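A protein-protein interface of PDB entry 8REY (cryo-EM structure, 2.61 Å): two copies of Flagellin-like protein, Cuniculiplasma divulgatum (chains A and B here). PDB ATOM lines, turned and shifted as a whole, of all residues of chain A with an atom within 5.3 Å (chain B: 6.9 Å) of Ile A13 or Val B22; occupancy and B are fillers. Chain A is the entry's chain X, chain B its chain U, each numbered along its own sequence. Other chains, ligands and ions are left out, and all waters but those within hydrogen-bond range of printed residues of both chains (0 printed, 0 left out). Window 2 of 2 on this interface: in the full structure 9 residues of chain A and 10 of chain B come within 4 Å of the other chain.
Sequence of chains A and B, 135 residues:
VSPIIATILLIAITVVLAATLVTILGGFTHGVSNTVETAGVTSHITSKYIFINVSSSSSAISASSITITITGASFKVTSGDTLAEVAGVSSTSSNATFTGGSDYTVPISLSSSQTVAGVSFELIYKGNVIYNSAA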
ATOM      1  N   LEU A   9       4.788  23.095  14.288  1.00  0.00           N
ATOM      2  CA  LEU A   9       5.686  23.108  15.440  1.00  0.00           C
ATOM      3  C   LEU A   9       5.122  23.931  16.606  1.00  0.00           C
ATOM      4  O   LEU A   9       5.192  23.485  17.752  1.00  0.00           O
ATOM      5  CB  LEU A   9       7.068  23.622  15.022  1.00  0.00           C
ATOM      6  CG  LEU A   9       7.850  22.749  14.042  1.00  0.00           C
ATOM      7  CD1 LEU A   9       9.103  23.471  13.576  1.00  0.00           C
ATOM      8  CD2 LEU A   9       8.218  21.410  14.662  1.00  0.00           C
ATOM      9  N   LEU A  10       4.530  25.103  16.329  1.00  0.00           N
ATOM     10  CA  LEU A  10       3.951  25.958  17.361  1.00  0.00           C
ATOM     11  C   LEU A  10       2.724  25.332  18.032  1.00  0.00           C
ATOM     12  O   LEU A  10       2.493  25.582  19.215  1.00  0.00           O
ATOM     13  CB  LEU A  10       3.611  27.332  16.778  1.00  0.00           C
ATOM     14  CG  LEU A  10       4.798  28.229  16.442  1.00  0.00           C
ATOM     15  CD1 LEU A  10       4.343  29.406  15.596  1.00  0.00           C
ATOM     16  CD2 LEU A  10       5.494  28.713  17.704  1.00  0.00           C
ATOM     17  N   ILE A  11       1.943  24.513  17.314  1.00  0.00           N
ATOM     18  CA  ILE A  11       0.831  23.788  17.920  1.00  0.00           C
ATOM     19  C   ILE A  11       1.364  22.736  18.892  1.00  0.00           C
ATOM     20  O   ILE A  11       0.904  22.677  20.030  1.00  0.00           O
ATOM     21  CB  ILE A  11      -0.139  23.233  16.858  1.00  0.00           C
ATOM     22  CG1 ILE A  11      -0.859  24.390  16.162  1.00  0.00           C
ATOM     23  CG2 ILE A  11      -1.135  22.239  17.456  1.00  0.00           C
ATOM     24  CD1 ILE A  11      -1.478  24.029  14.834  1.00  0.00           C
ATOM     25  N   ALA A  12       2.382  21.969  18.488  1.00  0.00           N
ATOM     26  CA  ALA A  12       3.019  20.987  19.355  1.00  0.00           C
ATOM     27  C   ALA A  12       3.552  21.613  20.654  1.00  0.00           C
ATOM     28  O   ALA A  12       3.328  21.064  21.730  1.00  0.00           O
ATOM     29  CB  ALA A  12       4.081  20.252  18.575  1.00  0.00           C
ATOM     30  N   ILE A  13       4.213  22.778  20.582  1.00  0.00           N
ATOM     31  CA  ILE A  13       4.701  23.499  21.757  1.00  0.00           C
ATOM     32  C   ILE A  13       3.542  23.961  22.652  1.00  0.00           C
ATOM     33  O   ILE A  13       3.634  23.868  23.875  1.00  0.00           O
ATOM     34  CB  ILE A  13       5.635  24.660  21.348  1.00  0.00           C
ATOM     35  CG1 ILE A  13       6.940  24.126  20.752  1.00  0.00           C
ATOM     36  CG2 ILE A  13       5.908  25.615  22.509  1.00  0.00           C
ATOM     37  CD1 ILE A  13       7.754  25.156  19.989  1.00  0.00           C
ATOM     38  N   THR A  14       2.441  24.432  22.055  1.00  0.00           N
ATOM     39  CA  THR A  14       1.294  24.961  22.786  1.00  0.00           C
ATOM     40  C   THR A  14       0.676  23.908  23.708  1.00  0.00           C
ATOM     41  O   THR A  14       0.369  24.209  24.857  1.00  0.00           O
ATOM     42  CB  THR A  14       0.237  25.533  21.833  1.00  0.00           C
ATOM     43  OG1 THR A  14       0.833  26.644  21.171  1.00  0.00           O
ATOM     44  CG2 THR A  14      -1.021  26.013  22.525  1.00  0.00           C
ATOM     45  N   VAL A  15       0.538  22.672  23.229  1.00  0.00           N
ATOM     46  CA  VAL A  15      -0.040  21.585  24.009  1.00  0.00           C
ATOM     47  C   VAL A  15       0.793  21.282  25.260  1.00  0.00           C
ATOM     48  O   VAL A  15       0.222  21.086  26.330  1.00  0.00           O
ATOM     49  CB  VAL A  15      -0.286  20.351  23.123  1.00  0.00           C
ATOM     50  CG1 VAL A  15      -0.703  19.121  23.916  1.00  0.00           C
ATOM     51  CG2 VAL A  15      -1.326  20.662  22.064  1.00  0.00           C
ATOM     52  N   VAL A  16       2.129  21.320  25.174  1.00  0.00           N
ATOM     53  CA  VAL A  16       2.994  21.040  26.318  1.00  0.00           C
ATOM     54  C   VAL A  16       2.909  22.153  27.373  1.00  0.00           C
ATOM     55  O   VAL A  16       2.956  21.872  28.572  1.00  0.00           O
ATOM     56  CB  VAL A  16       4.439  20.739  25.867  1.00  0.00           C
ATOM     57  CG1 VAL A  16       5.405  20.557  27.028  1.00  0.00           C
ATOM     58  CG2 VAL A  16       4.474  19.516  24.971  1.00  0.00           C
ATOM     59  N   LEU A  17       2.744  23.411  26.947  1.00  0.00           N
ATOM     60  CA  LEU A  17       2.541  24.511  27.881  1.00  0.00           C
ATOM     61  C   LEU A  17       1.211  24.367  28.621  1.00  0.00           C
ATOM     62  O   LEU A  17       1.181  24.516  29.838  1.00  0.00           O
ATOM     63  CB  LEU A  17       2.605  25.850  27.149  1.00  0.00           C
ATOM     64  CG  LEU A  17       3.958  26.213  26.549  1.00  0.00           C
ATOM     65  CD1 LEU A  17       3.807  27.431  25.657  1.00  0.00           C
ATOM     66  CD2 LEU A  17       4.998  26.479  27.628  1.00  0.00           C
ATOM     67  N   LEU B  17      15.309  27.965  14.775  1.00  0.00           N
ATOM     68  CA  LEU B  17      14.492  28.993  15.408  1.00  0.00           C
ATOM     69  C   LEU B  17      13.530  28.383  16.427  1.00  0.00           C
ATOM     70  O   LEU B  17      13.430  28.890  17.541  1.00  0.00           O
ATOM     71  CB  LEU B  17      13.726  29.789  14.354  1.00  0.00           C
ATOM     72  CG  LEU B  17      14.577  30.624  13.404  1.00  0.00           C
ATOM     73  CD1 LEU B  17      13.708  31.153  12.280  1.00  0.00           C
ATOM     74  CD2 LEU B  17      15.260  31.777  14.128  1.00  0.00           C
ATOM     75  N   ALA B  18      12.856  27.280  16.076  1.00  0.00           N
ATOM     76  CA  ALA B  18      11.955  26.589  16.987  1.00  0.00           C
ATOM     77  C   ALA B  18      12.700  26.079  18.229  1.00  0.00           C
ATOM     78  O   ALA B  18      12.241  26.275  19.351  1.00  0.00           O
ATOM     79  CB  ALA B  18      11.233  25.491  16.247  1.00  0.00           C
ATOM     80  N   ALA B  19      13.881  25.484  18.044  1.00  0.00           N
ATOM     81  CA  ALA B  19      14.723  25.047  19.149  1.00  0.00           C
ATOM     82  C   ALA B  19      15.161  26.222  20.032  1.00  0.00           C
ATOM     83  O   ALA B  19      15.231  26.080  21.247  1.00  0.00           O
ATOM     84  CB  ALA B  19      15.895  24.275  18.603  1.00  0.00           C
ATOM     85  N   THR B  20      15.425  27.396  19.443  1.00  0.00           N
ATOM     86  CA  THR B  20      15.756  28.600  20.198  1.00  0.00           C
ATOM     87  C   THR B  20      14.568  29.052  21.048  1.00  0.00           C
ATOM     88  O   THR B  20      14.734  29.273  22.243  1.00  0.00           O
ATOM     89  CB  THR B  20      16.234  29.732  19.278  1.00  0.00           C
ATOM     90  OG1 THR B  20      17.407  29.287  18.600  1.00  0.00           O
ATOM     91  CG2 THR B  20      16.547  31.020  20.008  1.00  0.00           C
ATOM     92  N   LEU B  21      13.370  29.144  20.454  1.00  0.00           N
ATOM     93  CA  LEU B  21      12.152  29.537  21.149  1.00  0.00           C
ATOM     94  C   LEU B  21      11.886  28.662  22.380  1.00  0.00           C
ATOM     95  O   LEU B  21      11.618  29.202  23.447  1.00  0.00           O
ATOM     96  CB  LEU B  21      10.980  29.537  20.164  1.00  0.00           C
ATOM     97  CG  LEU B  21       9.590  29.739  20.774  1.00  0.00           C
ATOM     98  CD1 LEU B  21       9.426  31.128  21.378  1.00  0.00           C
ATOM     99  CD2 LEU B  21       8.505  29.472  19.747  1.00  0.00           C
ATOM    100  N   VAL B  22      12.037  27.335  22.266  1.00  0.00           N
ATOM    101  CA  VAL B  22      11.849  26.405  23.375  1.00  0.00           C
ATOM    102  C   VAL B  22      12.728  26.767  24.577  1.00  0.00           C
ATOM    103  O   VAL B  22      12.265  26.693  25.712  1.00  0.00           O
ATOM    104  CB  VAL B  22      12.034  24.945  22.916  1.00  0.00           C
ATOM    105  CG1 VAL B  22      12.225  23.958  24.063  1.00  0.00           C
ATOM    106  CG2 VAL B  22      10.881  24.498  22.041  1.00  0.00           C
ATOM    107  N   THR B  23      13.966  27.228  24.364  1.00  0.00           N
ATOM    108  CA  THR B  23      14.815  27.624  25.483  1.00  0.00           C
ATOM    109  C   THR B  23      14.420  28.967  26.096  1.00  0.00           C
ATOM    110  O   THR B  23      14.676  29.182  27.279  1.00  0.00           O
ATOM    111  CB  THR B  23      16.309  27.615  25.147  1.00  0.00           C
ATOM    112  OG1 THR B  23      16.622  28.687  24.257  1.00  0.00           O
ATOM    113  CG2 THR B  23      16.771  26.295  24.577  1.00  0.00           C
ATOM    114  N   ILE B  24      13.786  29.862  25.330  1.00  0.00           N
ATOM    115  CA  ILE B  24      13.241  31.101  25.877  1.00  0.00           C
ATOM    116  C   ILE B  24      12.077  30.795  26.823  1.00  0.00           C
ATOM    117  O   ILE B  24      12.033  31.338  27.926  1.00  0.00           O
ATOM    118  CB  ILE B  24      12.862  32.098  24.760  1.00  0.00           C
ATOM    119  CG1 ILE B  24      14.102  32.539  23.977  1.00  0.00           C
ATOM    120  CG2 ILE B  24      12.082  33.290  25.308  1.00  0.00           C
ATOM    121  CD1 ILE B  24      13.811  33.292  22.692  1.00  0.00           C
ATOM    122  N   LEU B  25      11.170  29.887  26.433  1.00  0.00           N
ATOM    123  CA  LEU B  25       9.978  29.591  27.225  1.00  0.00           C
ATOM    124  C   LEU B  25      10.335  28.991  28.585  1.00  0.00           C
ATOM    125  O   LEU B  25       9.628  29.250  29.553  1.00  0.00           O
ATOM    126  CB  LEU B  25       9.012  28.668  26.478  1.00  0.00           C
ATOM    127  CG  LEU B  25       8.599  29.087  25.068  1.00  0.00           C
ATOM    128  CD1 LEU B  25       7.372  28.315  24.632  1.00  0.00           C
ATOM    129  CD2 LEU B  25       8.332  30.578  24.975  1.00  0.00           C
ATOM    130  N   GLY B  26      11.429  28.223  28.665  1.00  0.00           N
ATOM    131  CA  GLY B  26      11.875  27.592  29.900  1.00  0.00           C
ATOM    132  C   GLY B  26      12.139  28.564  31.056  1.00  0.00           C
ATOM    133  O   GLY B  26      12.150  28.145  32.207  1.00  0.00           O
ATOM    134  N   GLY B  27      12.332  29.859  30.772  1.00  0.00           N
ATOM    135  CA  GLY B  27      12.508  30.876  31.805  1.00  0.00           C
ATOM    136  C   GLY B  27      11.202  31.326  32.474  1.00  0.00           C
ATOM    137  O   GLY B  27      11.238  32.023  33.483  1.00  0.00           O
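O of Leu A10 sits at hydrogen-bond distance from OG1 of Thr A14 (2.8 Å).
Among the printed residues, merely in contact across the chains: Leu A9 with Ala B18 (3.97 Å), Leu A10 with Leu B21 (3.7 Å), Ile A13 with Val B22 (3.8 Å), Ile A13 with Leu B25 (3.7 Å) and Leu A17 with Leu B25 (3.8 Å).
Ile A13 touches just these residues of chain B: Val B22 and Leu B25. Val B22 touches just one residue of chain A: Ile A13 (3.8 Å). Of the printed residues of chain A, Ala B18 touches Leu A9 (3.97 Å). Of the printed residues of chain A, Leu B21 touches Leu A10. Printed residues of chain B within 4 Å of Leu A9: Ala B18 (3.97 Å). Ile B24 touches none of the printed residues of chain A.
Hydrophobic or aromatic side chains of chain A within 4 Å of the printed part of chain B: Leu A9, Leu A10, Ile A13 and Leu A17. Along chain A the printed residues that touch a printed residue of chain B span positions 9 to 17. Hydrophobic or aromatic side chains of chain B that line the printed part of chain A: Ala B18, Leu B21, Val B22 and Leu B25. Among the printed residues, 5 pairs touch across the chains. Among the printed residues, no Asp or Glu carboxylate lies within 4 Å of a Lys or Arg side-chain nitrogen of the other chain.
1 position is printed for both chains. Of the 5 pairs that touch across the chains among the printed residues, none has its exchanged pair printed and touching as well.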
